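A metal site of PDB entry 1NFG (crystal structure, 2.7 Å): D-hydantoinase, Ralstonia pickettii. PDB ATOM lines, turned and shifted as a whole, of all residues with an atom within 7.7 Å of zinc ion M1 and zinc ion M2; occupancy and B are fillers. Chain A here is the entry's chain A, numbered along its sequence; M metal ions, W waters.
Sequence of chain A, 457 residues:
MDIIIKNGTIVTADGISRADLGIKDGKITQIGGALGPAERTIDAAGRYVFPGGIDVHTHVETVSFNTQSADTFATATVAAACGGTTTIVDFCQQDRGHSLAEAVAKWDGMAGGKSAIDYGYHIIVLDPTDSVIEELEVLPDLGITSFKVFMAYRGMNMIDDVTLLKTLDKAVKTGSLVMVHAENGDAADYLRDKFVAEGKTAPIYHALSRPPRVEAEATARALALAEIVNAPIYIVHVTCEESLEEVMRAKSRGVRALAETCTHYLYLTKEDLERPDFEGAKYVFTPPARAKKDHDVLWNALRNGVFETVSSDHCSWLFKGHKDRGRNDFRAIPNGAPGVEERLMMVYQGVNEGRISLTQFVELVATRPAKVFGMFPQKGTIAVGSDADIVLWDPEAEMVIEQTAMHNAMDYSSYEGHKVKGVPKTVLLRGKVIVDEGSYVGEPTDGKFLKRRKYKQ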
ATOM      1  N   HIS A  57      37.491   3.287  14.448  1.00  0.00           N
ATOM      2  CA  HIS A  57      36.240   2.626  14.807  1.00  0.00           C
ATOM      3  C   HIS A  57      36.471   1.263  15.449  1.00  0.00           C
ATOM      4  O   HIS A  57      36.379   0.236  14.785  1.00  0.00           O
ATOM      5  CB  HIS A  57      35.351   2.471  13.571  1.00  0.00           C
ATOM      6  CG  HIS A  57      33.947   2.067  13.875  1.00  0.00           C
ATOM      7  ND1 HIS A  57      32.883   2.392  13.065  1.00  0.00           N
ATOM      8  CD2 HIS A  57      33.412   1.357  14.906  1.00  0.00           C
ATOM      9  CE1 HIS A  57      31.765   1.905  13.580  1.00  0.00           C
ATOM     10  NE2 HIS A  57      32.060   1.278  14.689  1.00  0.00           N
ATOM     11  N   THR A  58      36.779   1.270  16.745  1.00  0.00           N
ATOM     12  CA  THR A  58      37.014   0.037  17.487  1.00  0.00           C
ATOM     13  C   THR A  58      36.215  -0.057  18.781  1.00  0.00           C
ATOM     14  O   THR A  58      35.827   0.958  19.372  1.00  0.00           O
ATOM     15  CB  THR A  58      38.504  -0.142  17.869  1.00  0.00           C
ATOM     16  OG1 THR A  58      38.942   0.984  18.646  1.00  0.00           O
ATOM     17  CG2 THR A  58      39.361  -0.265  16.635  1.00  0.00           C
ATOM     18  N   HIS A  59      35.977  -1.296  19.198  1.00  0.00           N
ATOM     19  CA  HIS A  59      35.282  -1.606  20.440  1.00  0.00           C
ATOM     20  C   HIS A  59      36.181  -2.655  21.069  1.00  0.00           C
ATOM     21  O   HIS A  59      35.782  -3.813  21.273  1.00  0.00           O
ATOM     22  CB  HIS A  59      33.899  -2.169  20.142  1.00  0.00           C
ATOM     23  CG  HIS A  59      33.009  -1.226  19.379  1.00  0.00           C
ATOM     24  ND1 HIS A  59      32.663   0.021  19.861  1.00  0.00           N
ATOM     25  CD2 HIS A  59      32.417  -1.343  18.170  1.00  0.00           C
ATOM     26  CE1 HIS A  59      31.893   0.624  18.985  1.00  0.00           C
ATOM     27  NE2 HIS A  59      31.728  -0.174  17.950  1.00  0.00           N
ATOM     28  N   PHE A  91      35.566   3.485  21.186  1.00  0.00           N
ATOM     29  CA  PHE A  91      34.309   4.096  21.590  1.00  0.00           C
ATOM     30  C   PHE A  91      34.107   3.932  23.082  1.00  0.00           C
ATOM     31  O   PHE A  91      33.758   2.846  23.564  1.00  0.00           O
ATOM     32  CB  PHE A  91      33.140   3.461  20.816  1.00  0.00           C
ATOM     33  CG  PHE A  91      32.951   4.026  19.439  1.00  0.00           C
ATOM     34  CD1 PHE A  91      32.395   5.289  19.272  1.00  0.00           C
ATOM     35  CD2 PHE A  91      33.376   3.328  18.311  1.00  0.00           C
ATOM     36  CE1 PHE A  91      32.267   5.853  17.999  1.00  0.00           C
ATOM     37  CE2 PHE A  91      33.248   3.872  17.036  1.00  0.00           C
ATOM     38  CZ  PHE A  91      32.689   5.144  16.880  1.00  0.00           C
ATOM     39  N   ILE A 124      30.330   7.765  23.611  1.00  0.00           N
ATOM     40  CA  ILE A 124      28.993   7.316  23.276  1.00  0.00           C
ATOM     41  C   ILE A 124      28.014   7.852  24.313  1.00  0.00           C
ATOM     42  O   ILE A 124      28.188   7.638  25.510  1.00  0.00           O
ATOM     43  CB  ILE A 124      28.850   5.795  23.305  1.00  0.00           C
ATOM     44  CG1 ILE A 124      29.639   5.160  22.165  1.00  0.00           C
ATOM     45  CG2 ILE A 124      27.385   5.415  23.179  1.00  0.00           C
ATOM     46  CD1 ILE A 124      29.434   3.676  22.029  1.00  0.00           C
ATOM     47  N   KCX A 148      29.192  10.143  19.850  1.00  0.00           N
ATOM     48  CA  KCX A 148      28.524   9.093  19.111  1.00  0.00           C
ATOM     49  CB  KCX A 148      29.464   7.888  19.008  1.00  0.00           C
ATOM     50  CG  KCX A 148      28.734   6.596  18.858  1.00  0.00           C
ATOM     51  CD  KCX A 148      28.346   6.332  17.426  1.00  0.00           C
ATOM     52  CE  KCX A 148      29.161   5.157  17.031  1.00  0.00           C
ATOM     53  NZ  KCX A 148      28.395   4.136  16.401  1.00  0.00           N
ATOM     54  C   KCX A 148      27.179   8.668  19.718  1.00  0.00           C
ATOM     55  O   KCX A 148      27.085   8.422  20.930  1.00  0.00           O
ATOM     56  CX  KCX A 148      28.747   2.851  16.287  1.00  0.00           C
ATOM     57  OQ1 KCX A 148      27.930   2.109  15.680  1.00  0.00           O
ATOM     58  OQ2 KCX A 148      29.865   2.428  16.788  1.00  0.00           O
ATOM     59  N   VAL A 149      26.144   8.574  18.874  1.00  0.00           N
ATOM     60  CA  VAL A 149      24.814   8.156  19.306  1.00  0.00           C
ATOM     61  C   VAL A 149      24.268   7.042  18.410  1.00  0.00           C
ATOM     62  O   VAL A 149      24.720   6.857  17.281  1.00  0.00           O
ATOM     63  CB  VAL A 149      23.813   9.332  19.302  1.00  0.00           C
ATOM     64  CG1 VAL A 149      24.203  10.337  20.379  1.00  0.00           C
ATOM     65  CG2 VAL A 149      23.791  10.006  17.938  1.00  0.00           C
ATOM     66  N   PHE A 150      23.299   6.285  18.925  1.00  0.00           N
ATOM     67  CA  PHE A 150      22.703   5.185  18.183  1.00  0.00           C
ATOM     68  C   PHE A 150      21.226   5.418  17.864  1.00  0.00           C
ATOM     69  O   PHE A 150      20.467   5.914  18.703  1.00  0.00           O
ATOM     70  CB  PHE A 150      22.838   3.877  18.969  1.00  0.00           C
ATOM     71  CG  PHE A 150      24.240   3.358  19.034  1.00  0.00           C
ATOM     72  CD1 PHE A 150      25.206   4.015  19.787  1.00  0.00           C
ATOM     73  CD2 PHE A 150      24.603   2.216  18.316  1.00  0.00           C
ATOM     74  CE1 PHE A 150      26.536   3.540  19.823  1.00  0.00           C
ATOM     75  CE2 PHE A 150      25.922   1.741  18.348  1.00  0.00           C
ATOM     76  CZ  PHE A 150      26.889   2.408  19.102  1.00  0.00           C
ATOM     77  N   TYR A 153      18.886  -0.337  18.376  1.00  0.00           N
ATOM     78  CA  TYR A 153      19.137  -1.020  19.645  1.00  0.00           C
ATOM     79  C   TYR A 153      18.248  -0.473  20.764  1.00  0.00           C
ATOM     80  O   TYR A 153      18.725   0.208  21.667  1.00  0.00           O
ATOM     81  CB  TYR A 153      20.598  -0.891  20.050  1.00  0.00           C
ATOM     82  CG  TYR A 153      21.568  -1.459  19.039  1.00  0.00           C
ATOM     83  CD1 TYR A 153      21.360  -2.719  18.481  1.00  0.00           C
ATOM     84  CD2 TYR A 153      22.719  -0.757  18.673  1.00  0.00           C
ATOM     85  CE1 TYR A 153      22.283  -3.269  17.584  1.00  0.00           C
ATOM     86  CE2 TYR A 153      23.642  -1.297  17.777  1.00  0.00           C
ATOM     87  CZ  TYR A 153      23.418  -2.549  17.236  1.00  0.00           C
ATOM     88  OH  TYR A 153      24.344  -3.091  16.362  1.00  0.00           O
ATOM     89  N   VAL A 180      27.140   8.767  14.082  1.00  0.00           N
ATOM     90  CA  VAL A 180      25.893   8.072  14.291  1.00  0.00           C
ATOM     91  C   VAL A 180      25.753   6.714  13.608  1.00  0.00           C
ATOM     92  O   VAL A 180      26.159   6.531  12.463  1.00  0.00           O
ATOM     93  CB  VAL A 180      24.680   8.959  13.871  1.00  0.00           C
ATOM     94  CG1 VAL A 180      24.874   9.465  12.475  1.00  0.00           C
ATOM     95  CG2 VAL A 180      23.395   8.164  13.961  1.00  0.00           C
ATOM     96  N   HIS A 181      25.188   5.773  14.351  1.00  0.00           N
ATOM     97  CA  HIS A 181      24.902   4.425  13.865  1.00  0.00           C
ATOM     98  C   HIS A 181      23.496   4.615  13.289  1.00  0.00           C
ATOM     99  O   HIS A 181      22.534   4.768  14.037  1.00  0.00           O
ATOM    100  CB  HIS A 181      24.881   3.450  15.036  1.00  0.00           C
ATOM    101  CG  HIS A 181      24.384   2.089  14.680  1.00  0.00           C
ATOM    102  ND1 HIS A 181      25.210   0.987  14.646  1.00  0.00           N
ATOM    103  CD2 HIS A 181      23.145   1.638  14.367  1.00  0.00           C
ATOM    104  CE1 HIS A 181      24.501  -0.086  14.324  1.00  0.00           C
ATOM    105  NE2 HIS A 181      23.243   0.283  14.153  1.00  0.00           N
ATOM    106  N   ALA A 182      23.387   4.631  11.966  1.00  0.00           N
ATOM    107  CA  ALA A 182      22.085   4.876  11.334  1.00  0.00           C
ATOM    108  C   ALA A 182      21.280   3.690  10.843  1.00  0.00           C
ATOM    109  O   ALA A 182      21.480   3.170   9.745  1.00  0.00           O
ATOM    110  CB  ALA A 182      22.261   5.897  10.208  1.00  0.00           C
ATOM    111  N   GLU A 183      20.335   3.272  11.676  1.00  0.00           N
ATOM    112  CA  GLU A 183      19.420   2.190  11.339  1.00  0.00           C
ATOM    113  C   GLU A 183      18.141   2.558  12.049  1.00  0.00           C
ATOM    114  O   GLU A 183      18.181   3.151  13.127  1.00  0.00           O
ATOM    115  CB  GLU A 183      19.894   0.857  11.884  1.00  0.00           C
ATOM    116  CG  GLU A 183      20.748   0.069  10.950  1.00  0.00           C
ATOM    117  CD  GLU A 183      21.096  -1.260  11.561  1.00  0.00           C
ATOM    118  OE1 GLU A 183      21.520  -1.239  12.726  1.00  0.00           O
ATOM    119  OE2 GLU A 183      20.947  -2.309  10.907  1.00  0.00           O
ATOM    120  N   VAL A 236      28.844   6.406  10.483  1.00  0.00           N
ATOM    121  CA  VAL A 236      29.700   5.247  10.610  1.00  0.00           C
ATOM    122  C   VAL A 236      29.154   4.096   9.774  1.00  0.00           C
ATOM    123  O   VAL A 236      27.966   4.046   9.477  1.00  0.00           O
ATOM    124  CB  VAL A 236      29.836   4.782  12.097  1.00  0.00           C
ATOM    125  CG1 VAL A 236      30.332   5.930  12.958  1.00  0.00           C
ATOM    126  CG2 VAL A 236      28.516   4.245  12.615  1.00  0.00           C
ATOM    127  N   HIS A 237      30.041   3.180   9.409  1.00  0.00           N
ATOM    128  CA  HIS A 237      29.720   2.027   8.593  1.00  0.00           C
ATOM    129  C   HIS A 237      28.595   2.133   7.561  1.00  0.00           C
ATOM    130  O   HIS A 237      27.519   1.571   7.743  1.00  0.00           O
ATOM    131  CB  HIS A 237      29.486   0.789   9.487  1.00  0.00           C
ATOM    132  CG  HIS A 237      28.485   0.996  10.588  1.00  0.00           C
ATOM    133  ND1 HIS A 237      27.294   1.658  10.406  1.00  0.00           N
ATOM    134  CD2 HIS A 237      28.496   0.601  11.883  1.00  0.00           C
ATOM    135  CE1 HIS A 237      26.614   1.661  11.537  1.00  0.00           C
ATOM    136  NE2 HIS A 237      27.330   1.035  12.446  1.00  0.00           N
ATOM    137  N   GLU A 260      32.000   6.682   6.267  1.00  0.00           N
ATOM    138  CA  GLU A 260      33.089   5.713   6.215  1.00  0.00           C
ATOM    139  C   GLU A 260      32.491   4.337   5.909  1.00  0.00           C
ATOM    140  O   GLU A 260      31.269   4.196   5.803  1.00  0.00           O
ATOM    141  CB  GLU A 260      33.796   5.634   7.568  1.00  0.00           C
ATOM    142  CG  GLU A 260      32.828   5.381   8.748  1.00  0.00           C
ATOM    143  CD  GLU A 260      33.462   4.599   9.899  1.00  0.00           C
ATOM    144  OE1 GLU A 260      34.543   5.003  10.367  1.00  0.00           O
ATOM    145  OE2 GLU A 260      32.869   3.579  10.329  1.00  0.00           O
ATOM    146  N   CYS A 262      33.595  -0.186   6.393  1.00  0.00           N
ATOM    147  CA  CYS A 262      34.428  -1.071   7.175  1.00  0.00           C
ATOM    148  C   CYS A 262      34.812  -2.282   6.351  1.00  0.00           C
ATOM    149  O   CYS A 262      34.007  -2.828   5.599  1.00  0.00           O
ATOM    150  CB  CYS A 262      33.702  -1.457   8.474  1.00  0.00           C
ATOM    151  SG  CYS A 262      33.171  -0.023   9.484  1.00  0.00           S
ATOM    152  N   TYR A 265      32.556  -4.935   4.865  1.00  0.00           N
ATOM    153  CA  TYR A 265      31.523  -4.518   3.938  1.00  0.00           C
ATOM    154  C   TYR A 265      32.030  -4.470   2.501  1.00  0.00           C
ATOM    155  O   TYR A 265      31.288  -4.154   1.574  1.00  0.00           O
ATOM    156  CB  TYR A 265      30.949  -3.164   4.356  1.00  0.00           C
ATOM    157  CG  TYR A 265      30.216  -3.250   5.672  1.00  0.00           C
ATOM    158  CD1 TYR A 265      29.112  -4.090   5.817  1.00  0.00           C
ATOM    159  CD2 TYR A 265      30.642  -2.519   6.774  1.00  0.00           C
ATOM    160  CE1 TYR A 265      28.452  -4.207   7.037  1.00  0.00           C
ATOM    161  CE2 TYR A 265      29.988  -2.617   8.009  1.00  0.00           C
ATOM    162  CZ  TYR A 265      28.892  -3.464   8.125  1.00  0.00           C
ATOM    163  OH  TYR A 265      28.245  -3.560   9.341  1.00  0.00           O
ATOM    164  N   THR A 286      26.402  -5.696  12.588  1.00  0.00           N
ATOM    165  CA  THR A 286      25.442  -4.689  12.179  1.00  0.00           C
ATOM    166  C   THR A 286      26.059  -3.383  11.701  1.00  0.00           C
ATOM    167  O   THR A 286      27.006  -2.882  12.305  1.00  0.00           O
ATOM    168  CB  THR A 286      24.483  -4.399  13.355  1.00  0.00           C
ATOM    169  OG1 THR A 286      23.776  -5.591  13.698  1.00  0.00           O
ATOM    170  CG2 THR A 286      23.499  -3.297  13.000  1.00  0.00           C
ATOM    171  N   PRO A 287      25.525  -2.808  10.614  1.00  0.00           N
ATOM    172  CA  PRO A 287      24.403  -3.342   9.834  1.00  0.00           C
ATOM    173  C   PRO A 287      24.767  -4.686   9.221  1.00  0.00           C
ATOM    174  O   PRO A 287      25.937  -5.075   9.203  1.00  0.00           O
ATOM    175  CB  PRO A 287      24.150  -2.251   8.807  1.00  0.00           C
ATOM    176  CG  PRO A 287      24.445  -1.014   9.581  1.00  0.00           C
ATOM    177  CD  PRO A 287      25.741  -1.387  10.282  1.00  0.00           C
ATOM    178  N   SER A 312      37.419  -0.625  11.050  1.00  0.00           N
ATOM    179  CA  SER A 312      37.072  -2.035  11.267  1.00  0.00           C
ATOM    180  C   SER A 312      35.810  -2.371  12.078  1.00  0.00           C
ATOM    181  O   SER A 312      35.184  -3.401  11.831  1.00  0.00           O
ATOM    182  CB  SER A 312      38.257  -2.764  11.916  1.00  0.00           C
ATOM    183  OG  SER A 312      38.523  -2.266  13.227  1.00  0.00           O
ATOM    184  N   ASP A 313      35.428  -1.513  13.025  1.00  0.00           N
ATOM    185  CA  ASP A 313      34.278  -1.794  13.890  1.00  0.00           C
ATOM    186  C   ASP A 313      34.573  -3.141  14.565  1.00  0.00           C
ATOM    187  O   ASP A 313      33.727  -4.042  14.619  1.00  0.00           O
ATOM    188  CB  ASP A 313      32.972  -1.882  13.074  1.00  0.00           C
ATOM    189  CG  ASP A 313      31.717  -1.894  13.964  1.00  0.00           C
ATOM    190  OD1 ASP A 313      31.792  -1.400  15.118  1.00  0.00           O
ATOM    191  OD2 ASP A 313      30.658  -2.391  13.514  1.00  0.00           O
ATOM    192  N   HIS A 314      35.795  -3.242  15.069  1.00  0.00           N
ATOM    193  CA  HIS A 314      36.295  -4.438  15.743  1.00  0.00           C
ATOM    194  C   HIS A 314      35.553  -4.802  17.028  1.00  0.00           C
ATOM    195  O   HIS A 314      35.427  -3.993  17.958  1.00  0.00           O
ATOM    196  CB  HIS A 314      37.793  -4.259  16.070  1.00  0.00           C
ATOM    197  CG  HIS A 314      38.408  -5.435  16.751  1.00  0.00           C
ATOM    198  ND1 HIS A 314      38.812  -6.571  16.068  1.00  0.00           N
ATOM    199  CD2 HIS A 314      38.650  -5.681  18.062  1.00  0.00           C
ATOM    200  CE1 HIS A 314      39.272  -7.454  16.930  1.00  0.00           C
ATOM    201  NE2 HIS A 314      39.193  -6.945  18.140  1.00  0.00           N
ATOM    202  N   CYS A 315      35.072  -6.042  17.059  1.00  0.00           N
ATOM    203  CA  CYS A 315      34.357  -6.593  18.207  1.00  0.00           C
ATOM    204  C   CYS A 315      34.931  -7.977  18.472  1.00  0.00           C
ATOM    205  O   CYS A 315      35.557  -8.582  17.610  1.00  0.00           O
ATOM    206  CB  CYS A 315      32.860  -6.695  17.919  1.00  0.00           C
ATOM    207  SG  CYS A 315      32.016  -5.111  17.861  1.00  0.00           S
HETATM  208 ZN    ZN M   1      30.456   0.124  16.023  1.00  0.00          ZN
HETATM  209 ZN    ZN M   2      27.478   0.324  14.946  1.00  0.00          ZN
HETATM  210  O   HOH W   1      28.054  -1.329  17.817  1.00  0.00           O
HETATM  211  O   HOH W   2      27.993  -1.798  14.958  1.00  0.00           O
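O of His 314 lies within hydrogen-bond range of N of His 59 (3.0 Å). The side-chain carboxylate (OE2) of Glu 260 is in hydrogen-bond range of the backbone NH (N) of His 237 (3.0 Å). The side-chain carboxylate (OE1) of Glu 183 sits at hydrogen-bond distance from a ring nitrogen (NE2) of His 181. OQ1 of KCX 148 lies close to a ring nitrogen (NE2) of His 237, at 3.5 Å. The backbone NH (N) of His 181 is in hydrogen-bond range of the backbone carbonyl oxygen (O) of Val 149, at 3.2 Å. A ring nitrogen (ND1) of His 57 lies within hydrogen-bond range of the side-chain carboxylate (OE2) of Glu 260 (3.0 Å). A ring nitrogen (ND1) of His 181 lies close to a ring nitrogen (NE2) of His 237.
Four residues have an atom within 4 Å of zinc ion M1: His 57, His 59, KCX 148 and Asp 313.
Of the 24 residues printed, 3 come within 4 Å of zinc ion M2.
Zinc ion M1 is bound by the side-chain carboxylate (OD1) of Asp 313, a ring nitrogen (NE2) of His 59, a ring nitrogen (NE2) of His 57 and OQ2 of KCX 148. Zinc ion M1 has four donor atoms within binding distance.
OQ1 of KCX 148 is bound to zinc ion M2, at 2.0 Å. Zinc ion M2 is bound by water W2 (2.2 Å). A ring nitrogen (ND1) of His 181 binds zinc ion M2 (2.4 Å). Zinc ion M2 has three donor atoms within binding distance. Slightly farther from zinc ion M2 lies NE2 of His 237 (2.6 Å).
Water W2 bridges O of Thr 286 and OD2 of Asp 313.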
